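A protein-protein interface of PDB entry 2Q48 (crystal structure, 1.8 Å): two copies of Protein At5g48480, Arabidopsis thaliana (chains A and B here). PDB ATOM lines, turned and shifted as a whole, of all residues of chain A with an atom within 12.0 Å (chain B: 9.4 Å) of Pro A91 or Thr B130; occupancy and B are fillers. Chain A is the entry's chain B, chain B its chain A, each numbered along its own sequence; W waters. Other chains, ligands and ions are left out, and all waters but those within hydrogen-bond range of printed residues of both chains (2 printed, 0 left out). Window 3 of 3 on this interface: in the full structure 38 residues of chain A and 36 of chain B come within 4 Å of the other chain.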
ATOM      1  N   MET A  29      14.472 -30.682  16.643  1.00  0.00           N
ATOM      2  CA  MET A  29      14.996 -30.402  15.309  1.00  0.00           C
ATOM      3  C   MET A  29      16.439 -29.945  15.458  1.00  0.00           C
ATOM      4  O   MET A  29      16.712 -28.926  16.130  1.00  0.00           O
ATOM      5  CB  MET A  29      14.169 -29.281  14.649  1.00  0.00           C
ATOM      6  CG  MET A  29      12.749 -29.743  14.335  1.00  0.00           C
ATOM      7  SD  MET A  29      11.601 -28.313  13.723  1.00  0.00           S
ATOM      8  CE  MET A  29      13.033 -27.562  12.435  1.00  0.00           C
ATOM      9  N   LEU A  31      19.517 -28.303  13.732  1.00  0.00           N
ATOM     10  CA  LEU A  31      19.791 -27.474  12.544  1.00  0.00           C
ATOM     11  C   LEU A  31      21.274 -27.611  12.164  1.00  0.00           C
ATOM     12  O   LEU A  31      22.135 -27.389  13.030  1.00  0.00           O
ATOM     13  CB  LEU A  31      19.545 -26.003  12.857  1.00  0.00           C
ATOM     14  CG  LEU A  31      18.068 -25.616  13.188  1.00  0.00           C
ATOM     15  CD1 LEU A  31      18.055 -24.288  13.949  1.00  0.00           C
ATOM     16  CD2 LEU A  31      17.249 -25.521  11.891  1.00  0.00           C
ATOM     17  N   VAL A  32      21.550 -27.947  10.903  1.00  0.00           N
ATOM     18  CA  VAL A  32      22.941 -28.071  10.443  1.00  0.00           C
ATOM     19  C   VAL A  32      23.190 -27.248   9.162  1.00  0.00           C
ATOM     20  O   VAL A  32      22.241 -26.805   8.489  1.00  0.00           O
ATOM     21  CB  VAL A  32      23.355 -29.520  10.151  1.00  0.00           C
ATOM     22  CG1 VAL A  32      23.160 -30.391  11.440  1.00  0.00           C
ATOM     23  CG2 VAL A  32      22.525 -30.071   9.001  1.00  0.00           C
ATOM     24  N   GLU A  33      24.484 -27.068   8.899  1.00  0.00           N
ATOM     25  CA  GLU A  33      25.019 -26.322   7.749  1.00  0.00           C
ATOM     26  C   GLU A  33      24.339 -26.653   6.403  1.00  0.00           C
ATOM     27  O   GLU A  33      24.000 -27.791   6.120  1.00  0.00           O
ATOM     28  CB  GLU A  33      26.553 -26.633   7.651  1.00  0.00           C
ATOM     29  CG  GLU A  33      27.159 -26.076   6.363  1.00  0.00           C
ATOM     30  CD  GLU A  33      28.676 -26.272   6.174  1.00  0.00           C
ATOM     31  OE1 GLU A  33      29.197 -27.426   6.221  1.00  0.00           O
ATOM     32  OE2 GLU A  33      29.354 -25.242   5.888  1.00  0.00           O
ATOM     33  N   ALA A  34      24.166 -25.649   5.539  1.00  0.00           N
ATOM     34  CA  ALA A  34      23.608 -25.912   4.224  1.00  0.00           C
ATOM     35  C   ALA A  34      24.376 -27.064   3.542  1.00  0.00           C
ATOM     36  O   ALA A  34      25.617 -27.174   3.647  1.00  0.00           O
ATOM     37  CB  ALA A  34      23.679 -24.610   3.327  1.00  0.00           C
ATOM     38  N   LEU A  71      16.957 -32.538   2.484  1.00  0.00           N
ATOM     39  CA  LEU A  71      16.418 -31.393   3.179  1.00  0.00           C
ATOM     40  C   LEU A  71      16.261 -31.705   4.672  1.00  0.00           C
ATOM     41  O   LEU A  71      16.364 -30.811   5.510  1.00  0.00           O
ATOM     42  CB  LEU A  71      15.055 -31.033   2.589  1.00  0.00           C
ATOM     43  CG  LEU A  71      14.283 -29.798   3.083  1.00  0.00           C
ATOM     44  CD1 LEU A  71      13.266 -29.388   2.009  1.00  0.00           C
ATOM     45  CD2 LEU A  71      13.577 -30.072   4.397  1.00  0.00           C
ATOM     46  N   CYS A  85      18.091 -31.184  10.090  1.00  0.00           N
ATOM     47  CA  CYS A  85      17.623 -30.468   8.929  1.00  0.00           C
ATOM     48  C   CYS A  85      18.477 -29.283   8.540  1.00  0.00           C
ATOM     49  O   CYS A  85      18.739 -28.421   9.347  1.00  0.00           O
ATOM     50  CB  CYS A  85      16.274 -29.955   9.188  1.00  0.00           C
ATOM     51  SG  CYS A  85      16.319 -28.794  10.477  1.00  0.00           S
ATOM     52  N   ASP A  86      18.873 -29.268   7.270  1.00  0.00           N
ATOM     53  CA  ASP A  86      19.699 -28.187   6.689  1.00  0.00           C
ATOM     54  C   ASP A  86      19.049 -26.818   6.999  1.00  0.00           C
ATOM     55  O   ASP A  86      17.907 -26.621   6.651  1.00  0.00           O
ATOM     56  CB  ASP A  86      19.665 -28.462   5.198  1.00  0.00           C
ATOM     57  CG  ASP A  86      20.407 -27.433   4.363  1.00  0.00           C
ATOM     58  OD1 ASP A  86      20.481 -26.241   4.738  1.00  0.00           O
ATOM     59  OD2 ASP A  86      20.922 -27.898   3.334  1.00  0.00           O
ATOM     60  N   VAL A  87      19.757 -25.872   7.611  1.00  0.00           N
ATOM     61  CA  VAL A  87      19.102 -24.583   7.939  1.00  0.00           C
ATOM     62  C   VAL A  87      18.760 -23.759   6.681  1.00  0.00           C
ATOM     63  O   VAL A  87      17.767 -23.027   6.632  1.00  0.00           O
ATOM     64  CB  VAL A  87      20.014 -23.770   8.892  1.00  0.00           C
ATOM     65  CG1 VAL A  87      21.267 -23.311   8.122  1.00  0.00           C
ATOM     66  CG2 VAL A  87      19.269 -22.602   9.505  1.00  0.00           C
ATOM     67  N   SER A  88      19.551 -23.907   5.633  1.00  0.00           N
ATOM     68  CA  SER A  88      19.250 -23.128   4.402  1.00  0.00           C
ATOM     69  C   SER A  88      17.793 -23.347   3.944  1.00  0.00           C
ATOM     70  O   SER A  88      17.244 -22.609   3.117  1.00  0.00           O
ATOM     71  CB  SER A  88      20.237 -23.475   3.290  1.00  0.00           C
ATOM     72  OG  SER A  88      20.206 -24.848   2.906  1.00  0.00           O
ATOM     73  N   SER A  89      17.148 -24.392   4.460  1.00  0.00           N
ATOM     74  CA  SER A  89      15.749 -24.632   4.130  1.00  0.00           C
ATOM     75  C   SER A  89      14.804 -23.879   5.063  1.00  0.00           C
ATOM     76  O   SER A  89      13.572 -23.898   4.846  1.00  0.00           O
ATOM     77  CB  SER A  89      15.383 -26.155   4.258  1.00  0.00           C
ATOM     78  OG  SER A  89      15.322 -26.521   5.659  1.00  0.00           O
ATOM     79  N   LEU A  90      15.362 -23.242   6.096  1.00  0.00           N
ATOM     80  CA  LEU A  90      14.557 -22.544   7.112  1.00  0.00           C
ATOM     81  C   LEU A  90      15.187 -21.198   7.392  1.00  0.00           C
ATOM     82  O   LEU A  90      15.950 -21.070   8.325  1.00  0.00           O
ATOM     83  CB  LEU A  90      14.580 -23.358   8.447  1.00  0.00           C
ATOM     84  CG  LEU A  90      13.749 -24.644   8.407  1.00  0.00           C
ATOM     85  CD1 LEU A  90      14.177 -25.617   9.530  1.00  0.00           C
ATOM     86  CD2 LEU A  90      12.272 -24.254   8.535  1.00  0.00           C
ATOM     87  N   PRO A  91      14.861 -20.181   6.563  1.00  0.00           N
ATOM     88  CA  PRO A  91      15.396 -18.818   6.716  1.00  0.00           C
ATOM     89  C   PRO A  91      14.965 -18.165   8.006  1.00  0.00           C
ATOM     90  O   PRO A  91      13.794 -18.261   8.403  1.00  0.00           O
ATOM     91  CB  PRO A  91      14.856 -18.080   5.472  1.00  0.00           C
ATOM     92  CG  PRO A  91      13.475 -18.823   5.247  1.00  0.00           C
ATOM     93  CD  PRO A  91      13.884 -20.286   5.470  1.00  0.00           C
ATOM     94  N   GLY A  92      15.908 -17.475   8.660  1.00  0.00           N
ATOM     95  CA  GLY A  92      15.597 -16.838   9.920  1.00  0.00           C
ATOM     96  C   GLY A  92      16.302 -17.613  11.018  1.00  0.00           C
ATOM     97  O   GLY A  92      16.838 -16.983  11.914  1.00  0.00           O
ATOM     98  N   PHE A  93      16.351 -18.946  10.921  1.00  0.00           N
ATOM     99  CA  PHE A  93      17.011 -19.773  11.939  1.00  0.00           C
ATOM    100  C   PHE A  93      18.512 -19.717  11.844  1.00  0.00           C
ATOM    101  O   PHE A  93      19.069 -19.344  10.815  1.00  0.00           O
ATOM    102  CB  PHE A  93      16.613 -21.264  11.779  1.00  0.00           C
ATOM    103  CG  PHE A  93      15.278 -21.612  12.385  1.00  0.00           C
ATOM    104  CD1 PHE A  93      15.186 -22.003  13.727  1.00  0.00           C
ATOM    105  CD2 PHE A  93      14.147 -21.590  11.610  1.00  0.00           C
ATOM    106  CE1 PHE A  93      13.942 -22.391  14.287  1.00  0.00           C
ATOM    107  CE2 PHE A  93      12.885 -21.972  12.145  1.00  0.00           C
ATOM    108  CZ  PHE A  93      12.800 -22.375  13.499  1.00  0.00           C
ATOM    109  N   SER A  94      19.164 -20.124  12.928  1.00  0.00           N
ATOM    110  CA  SER A  94      20.619 -20.139  12.938  1.00  0.00           C
ATOM    111  C   SER A  94      21.048 -21.438  13.633  1.00  0.00           C
ATOM    112  O   SER A  94      20.501 -21.789  14.705  1.00  0.00           O
ATOM    113  CB  SER A  94      21.163 -18.952  13.756  1.00  0.00           C
ATOM    114  OG  SER A  94      22.556 -19.075  13.872  1.00  0.00           O
ATOM    115  N   THR A  95      21.980 -22.145  13.027  1.00  0.00           N
ATOM    116  CA  THR A  95      22.522 -23.368  13.619  1.00  0.00           C
ATOM    117  C   THR A  95      23.222 -23.036  14.966  1.00  0.00           C
ATOM    118  O   THR A  95      23.337 -23.901  15.819  1.00  0.00           O
ATOM    119  CB  THR A  95      23.652 -23.973  12.769  1.00  0.00           C
ATOM    120  OG1 THR A  95      24.740 -23.020  12.657  1.00  0.00           O
ATOM    121  CG2 THR A  95      23.106 -24.396  11.386  1.00  0.00           C
ATOM    122  N   ALA A  96      23.719 -21.806  15.084  1.00  0.00           N
ATOM    123  CA  ALA A  96      24.476 -21.325  16.270  1.00  0.00           C
ATOM    124  C   ALA A  96      25.752 -22.133  16.441  1.00  0.00           C
ATOM    125  O   ALA A  96      26.372 -22.138  17.523  1.00  0.00           O
ATOM    126  CB  ALA A  96      23.596 -21.409  17.559  1.00  0.00           C
ATOM    127  N   VAL B 127       6.414 -15.504  16.520  1.00  0.00           N
ATOM    128  CA  VAL B 127       7.303 -15.115  15.414  1.00  0.00           C
ATOM    129  C   VAL B 127       6.488 -15.429  14.136  1.00  0.00           C
ATOM    130  O   VAL B 127       5.911 -16.515  14.015  1.00  0.00           O
ATOM    131  CB  VAL B 127       8.617 -15.988  15.374  1.00  0.00           C
ATOM    132  CG1 VAL B 127       9.456 -15.633  14.152  1.00  0.00           C
ATOM    133  CG2 VAL B 127       9.474 -15.787  16.647  1.00  0.00           C
ATOM    134  N   GLU B 128       6.456 -14.493  13.183  1.00  0.00           N
ATOM    135  CA  GLU B 128       5.711 -14.711  11.955  1.00  0.00           C
ATOM    136  C   GLU B 128       6.340 -15.861  11.196  1.00  0.00           C
ATOM    137  O   GLU B 128       7.565 -15.927  11.074  1.00  0.00           O
ATOM    138  CB  GLU B 128       5.766 -13.436  11.077  1.00  0.00           C
ATOM    139  CG  GLU B 128       5.063 -12.227  11.699  1.00  0.00           C
ATOM    140  CD  GLU B 128       3.556 -12.401  11.743  1.00  0.00           C
ATOM    141  OE1 GLU B 128       2.972 -12.723  10.670  1.00  0.00           O
ATOM    142  OE2 GLU B 128       2.955 -12.218  12.837  1.00  0.00           O
ATOM    143  N   VAL B 129       5.509 -16.772  10.701  1.00  0.00           N
ATOM    144  CA  VAL B 129       5.991 -17.927   9.967  1.00  0.00           C
ATOM    145  C   VAL B 129       6.217 -17.548   8.515  1.00  0.00           C
ATOM    146  O   VAL B 129       5.310 -17.100   7.829  1.00  0.00           O
ATOM    147  CB  VAL B 129       4.986 -19.062  10.010  1.00  0.00           C
ATOM    148  CG1 VAL B 129       4.806 -19.523  11.477  1.00  0.00           C
ATOM    149  CG2 VAL B 129       3.619 -18.570   9.472  1.00  0.00           C
ATOM    150  N   THR B 130       7.436 -17.723   8.067  1.00  0.00           N
ATOM    151  CA  THR B 130       7.807 -17.358   6.679  1.00  0.00           C
ATOM    152  C   THR B 130       6.916 -18.103   5.703  1.00  0.00           C
ATOM    153  O   THR B 130       6.254 -19.088   6.060  1.00  0.00           O
ATOM    154  CB  THR B 130       9.204 -17.807   6.428  1.00  0.00           C
ATOM    155  OG1 THR B 130       9.294 -19.205   6.714  1.00  0.00           O
ATOM    156  CG2 THR B 130      10.147 -17.063   7.362  1.00  0.00           C
ATOM    157  N   GLU B 131       6.940 -17.666   4.453  1.00  0.00           N
ATOM    158  CA  GLU B 131       6.136 -18.363   3.464  1.00  0.00           C
ATOM    159  C   GLU B 131       6.616 -19.797   3.443  1.00  0.00           C
ATOM    160  O   GLU B 131       5.814 -20.731   3.453  1.00  0.00           O
ATOM    161  CB  GLU B 131       6.263 -17.668   2.111  1.00  0.00           C
ATOM    162  CG  GLU B 131       5.232 -18.251   1.115  1.00  0.00           C
ATOM    163  CD  GLU B 131       5.768 -19.481   0.537  1.00  0.00           C
ATOM    164  OE1 GLU B 131       6.986 -19.683   0.751  1.00  0.00           O
ATOM    165  OE2 GLU B 131       5.034 -20.239  -0.151  1.00  0.00           O
ATOM    166  N   ALA B 132       7.945 -19.926   3.475  1.00  0.00           N
ATOM    167  CA  ALA B 132       8.695 -21.160   3.513  1.00  0.00           C
ATOM    168  C   ALA B 132       8.123 -22.088   4.628  1.00  0.00           C
ATOM    169  O   ALA B 132       7.712 -23.207   4.372  1.00  0.00           O
ATOM    170  CB  ALA B 132      10.139 -20.846   3.849  1.00  0.00           C
ATOM    171  N   GLU B 133       8.198 -21.628   5.880  1.00  0.00           N
ATOM    172  CA  GLU B 133       7.675 -22.474   6.989  1.00  0.00           C
ATOM    173  C   GLU B 133       6.218 -22.933   6.704  1.00  0.00           C
ATOM    174  O   GLU B 133       5.788 -24.084   7.020  1.00  0.00           O
ATOM    175  CB  GLU B 133       7.739 -21.675   8.299  1.00  0.00           C
ATOM    176  CG  GLU B 133       9.164 -21.644   8.766  1.00  0.00           C
ATOM    177  CD  GLU B 133       9.428 -20.641   9.873  1.00  0.00           C
ATOM    178  OE1 GLU B 133       8.578 -19.764  10.136  1.00  0.00           O
ATOM    179  OE2 GLU B 133      10.526 -20.752  10.446  1.00  0.00           O
ATOM    180  N   VAL B 134       5.429 -22.027   6.156  1.00  0.00           N
ATOM    181  CA  VAL B 134       4.048 -22.425   5.855  1.00  0.00           C
ATOM    182  C   VAL B 134       3.981 -23.542   4.797  1.00  0.00           C
ATOM    183  O   VAL B 134       3.005 -24.326   4.761  1.00  0.00           O
ATOM    184  CB  VAL B 134       3.183 -21.263   5.379  1.00  0.00           C
ATOM    185  CG1 VAL B 134       1.737 -21.796   5.157  1.00  0.00           C
ATOM    186  CG2 VAL B 134       3.149 -20.154   6.406  1.00  0.00           C
ATOM    187  N   GLU B 135       4.996 -23.636   3.936  1.00  0.00           N
ATOM    188  CA  GLU B 135       5.003 -24.687   2.910  1.00  0.00           C
ATOM    189  C   GLU B 135       5.260 -26.077   3.509  1.00  0.00           C
ATOM    190  O   GLU B 135       4.845 -27.092   2.923  1.00  0.00           O
ATOM    191  CB  GLU B 135       6.040 -24.383   1.827  1.00  0.00           C
ATOM    192  CG  GLU B 135       5.768 -23.052   1.105  1.00  0.00           C
ATOM    193  CD  GLU B 135       6.760 -22.742  -0.018  1.00  0.00           C
ATOM    194  OE1 GLU B 135       7.998 -22.900   0.191  1.00  0.00           O
ATOM    195  OE2 GLU B 135       6.299 -22.309  -1.095  1.00  0.00           O
ATOM    196  N   LEU B 136       5.977 -26.121   4.641  1.00  0.00           N
ATOM    197  CA  LEU B 136       6.275 -27.386   5.333  1.00  0.00           C
ATOM    198  C   LEU B 136       5.139 -27.692   6.327  1.00  0.00           C
ATOM    199  O   LEU B 136       5.195 -28.659   7.115  1.00  0.00           O
ATOM    200  CB  LEU B 136       7.662 -27.308   6.050  1.00  0.00           C
ATOM    201  CG  LEU B 136       8.902 -27.260   5.139  1.00  0.00           C
ATOM    202  CD1 LEU B 136      10.216 -26.886   5.863  1.00  0.00           C
ATOM    203  CD2 LEU B 136       9.021 -28.624   4.470  1.00  0.00           C
ATOM    204  N   GLY B 137       4.098 -26.872   6.284  1.00  0.00           N
ATOM    205  CA  GLY B 137       2.952 -27.047   7.185  1.00  0.00           C
ATOM    206  C   GLY B 137       3.152 -26.411   8.555  1.00  0.00           C
ATOM    207  O   GLY B 137       2.258 -26.474   9.418  1.00  0.00           O
ATOM    208  N   PHE B 138       4.330 -25.808   8.761  1.00  0.00           N
ATOM    209  CA  PHE B 138       4.678 -25.164  10.052  1.00  0.00           C
ATOM    210  C   PHE B 138       3.912 -23.862  10.096  1.00  0.00           C
ATOM    211  O   PHE B 138       4.417 -22.815   9.652  1.00  0.00           O
ATOM    212  CB  PHE B 138       6.181 -24.877  10.145  1.00  0.00           C
ATOM    213  CG  PHE B 138       7.019 -26.087  10.330  1.00  0.00           C
ATOM    214  CD1 PHE B 138       6.692 -27.047  11.308  1.00  0.00           C
ATOM    215  CD2 PHE B 138       8.172 -26.273   9.579  1.00  0.00           C
ATOM    216  CE1 PHE B 138       7.510 -28.151  11.495  1.00  0.00           C
ATOM    217  CE2 PHE B 138       8.984 -27.376   9.770  1.00  0.00           C
ATOM    218  CZ  PHE B 138       8.662 -28.318  10.720  1.00  0.00           C
ATOM    219  N   LYS B 139       2.705 -23.915  10.666  1.00  0.00           N
ATOM    220  CA  LYS B 139       1.797 -22.777  10.684  1.00  0.00           C
ATOM    221  C   LYS B 139       1.954 -21.751  11.804  1.00  0.00           C
ATOM    222  O   LYS B 139       1.481 -20.598  11.692  1.00  0.00           O
ATOM    223  CB  LYS B 139       0.339 -23.294  10.648  1.00  0.00           C
ATOM    224  CG  LYS B 139      -0.066 -23.965   9.323  1.00  0.00           C
ATOM    225  CD  LYS B 139       0.006 -22.980   8.157  1.00  0.00           C
ATOM    226  CE  LYS B 139      -0.226 -23.661   6.803  1.00  0.00           C
ATOM    227  NZ  LYS B 139      -1.571 -24.275   6.646  1.00  0.00           N
ATOM    228  N   GLY B 140       2.605 -22.145  12.895  1.00  0.00           N
ATOM    229  CA  GLY B 140       2.802 -21.203  13.992  1.00  0.00           C
ATOM    230  C   GLY B 140       4.221 -21.391  14.526  1.00  0.00           C
ATOM    231  O   GLY B 140       4.825 -22.434  14.320  1.00  0.00           O
ATOM    232  N   LYS B 141       4.733 -20.382  15.240  1.00  0.00           N
ATOM    233  CA  LYS B 141       6.110 -20.435  15.734  1.00  0.00           C
ATOM    234  C   LYS B 141       6.276 -19.423  16.880  1.00  0.00           C
ATOM    235  O   LYS B 141       5.726 -18.335  16.811  1.00  0.00           O
ATOM    236  CB  LYS B 141       7.022 -20.030  14.562  1.00  0.00           C
ATOM    237  CG  LYS B 141       8.428 -19.807  14.900  1.00  0.00           C
ATOM    238  CD  LYS B 141       9.168 -19.458  13.553  1.00  0.00           C
ATOM    239  CE  LYS B 141      10.646 -19.280  13.744  1.00  0.00           C
ATOM    240  NZ  LYS B 141      11.258 -18.916  12.394  1.00  0.00           N
ATOM    241  N   THR B 149      13.162 -22.358  20.535  1.00  0.00           N
ATOM    242  CA  THR B 149      12.271 -22.049  19.430  1.00  0.00           C
ATOM    243  C   THR B 149      11.390 -23.270  19.266  1.00  0.00           C
ATOM    244  O   THR B 149      11.887 -24.413  19.100  1.00  0.00           O
ATOM    245  CB  THR B 149      13.038 -21.845  18.103  1.00  0.00           C
ATOM    246  OG1 THR B 149      13.994 -20.767  18.299  1.00  0.00           O
ATOM    247  CG2 THR B 149      12.096 -21.427  17.031  1.00  0.00           C
ATOM    248  N   ILE B 151       8.112 -24.710  16.975  1.00  0.00           N
ATOM    249  CA  ILE B 151       7.328 -24.414  15.754  1.00  0.00           C
ATOM    250  C   ILE B 151       6.227 -25.452  15.730  1.00  0.00           C
ATOM    251  O   ILE B 151       6.491 -26.611  16.016  1.00  0.00           O
ATOM    252  CB  ILE B 151       8.182 -24.602  14.511  1.00  0.00           C
ATOM    253  CG1 ILE B 151       9.591 -24.098  14.793  1.00  0.00           C
ATOM    254  CG2 ILE B 151       7.480 -23.945  13.243  1.00  0.00           C
ATOM    255  CD1 ILE B 151       9.680 -22.593  15.223  1.00  0.00           C
HETATM  256  O   HOH W   1      12.115 -17.364  10.513  1.00  0.00           O
HETATM  257  O   HOH W   2      11.971 -20.252   8.005  1.00  0.00           O
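O of Lys B141 lies within hydrogen-bond range of N of Val B127 (2.9 Å).
The backbone NH (N) of Glu B133 sits at hydrogen-bond distance from the side-chain hydroxyl (OG1) of Thr B130 (2.8 Å).
O of Glu B133 is in hydrogen-bond range of N of Phe B138 (2.9 Å).
The side-chain amino group (NZ) of Lys B141 lies within salt-bridge range of the side-chain carboxylate (OE2) of Glu B133 (2.8 Å).
Among the printed residues, pairs that only touch across the chains: Phe A93 with Glu B133, Phe A93 with Thr B149, Phe A93 with Lys B141, Phe A93 with Ile B151 and Pro A91 with Thr B130.
Pro A91 touches just one residue of chain B: Thr B130.
Of chain A, only Pro A91 comes within 4 Å of Thr B130.
No residue of chain B comes within 4 Å of Gly A92.
No residue of chain A comes within 4 Å of Val B129.
No residue of chain A comes within 4 Å of Glu B131.
No residue of chain A comes within 4 Å of Ala B132.
Glu B133 touches just one residue of chain A: Phe A93 (3.2 Å).
Of the printed residues of chain B, Phe A93 touches Glu B133 (3.2 Å), Lys B141 (3.5 Å), Thr B149 (3.4 Å) and Ile B151 (3.6 Å).
Printed residues of chain A within 4 Å of Thr B149: Phe A93 (3.4 Å).
Ser A89 touches none of the printed residues of chain B.
The nearest residue of chain A that does not touch Thr B130 is Gly A92 (5.9 Å).
The nearest printed residue of chain A that does not touch Lys B141 is Pro A91 (4.8 Å).
Of the 17 printed residues of chain B, 5 touch a printed residue of chain A.
Printed residues of chain B that touch a printed residue of chain A: Thr B130, Glu B133, Lys B141, Thr B149 and Ile B151.
Hydrophobic or aromatic side chains of chain B within 4 Å of the printed part of chain A: Ile B151.
Among the printed residues, 5 pairs touch across the chains.
Among the printed residues, no Asp or Glu carboxylate lies within 4 Å of a Lys or Arg side-chain nitrogen of the other chain.
No position is printed for both chains.
Water W1 bridges NZ of Lys B141 (2.6 Å) and O of Pro A91 (2.8 Å).
Water W2 lies within hydrogen-bond range of the backbone carbonyl oxygen of Pro A91 (2.7 Å), the side-chain carboxylate of Glu B133 (2.9 Å) and the side-chain hydroxyl of Thr B130 (3.2 Å).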
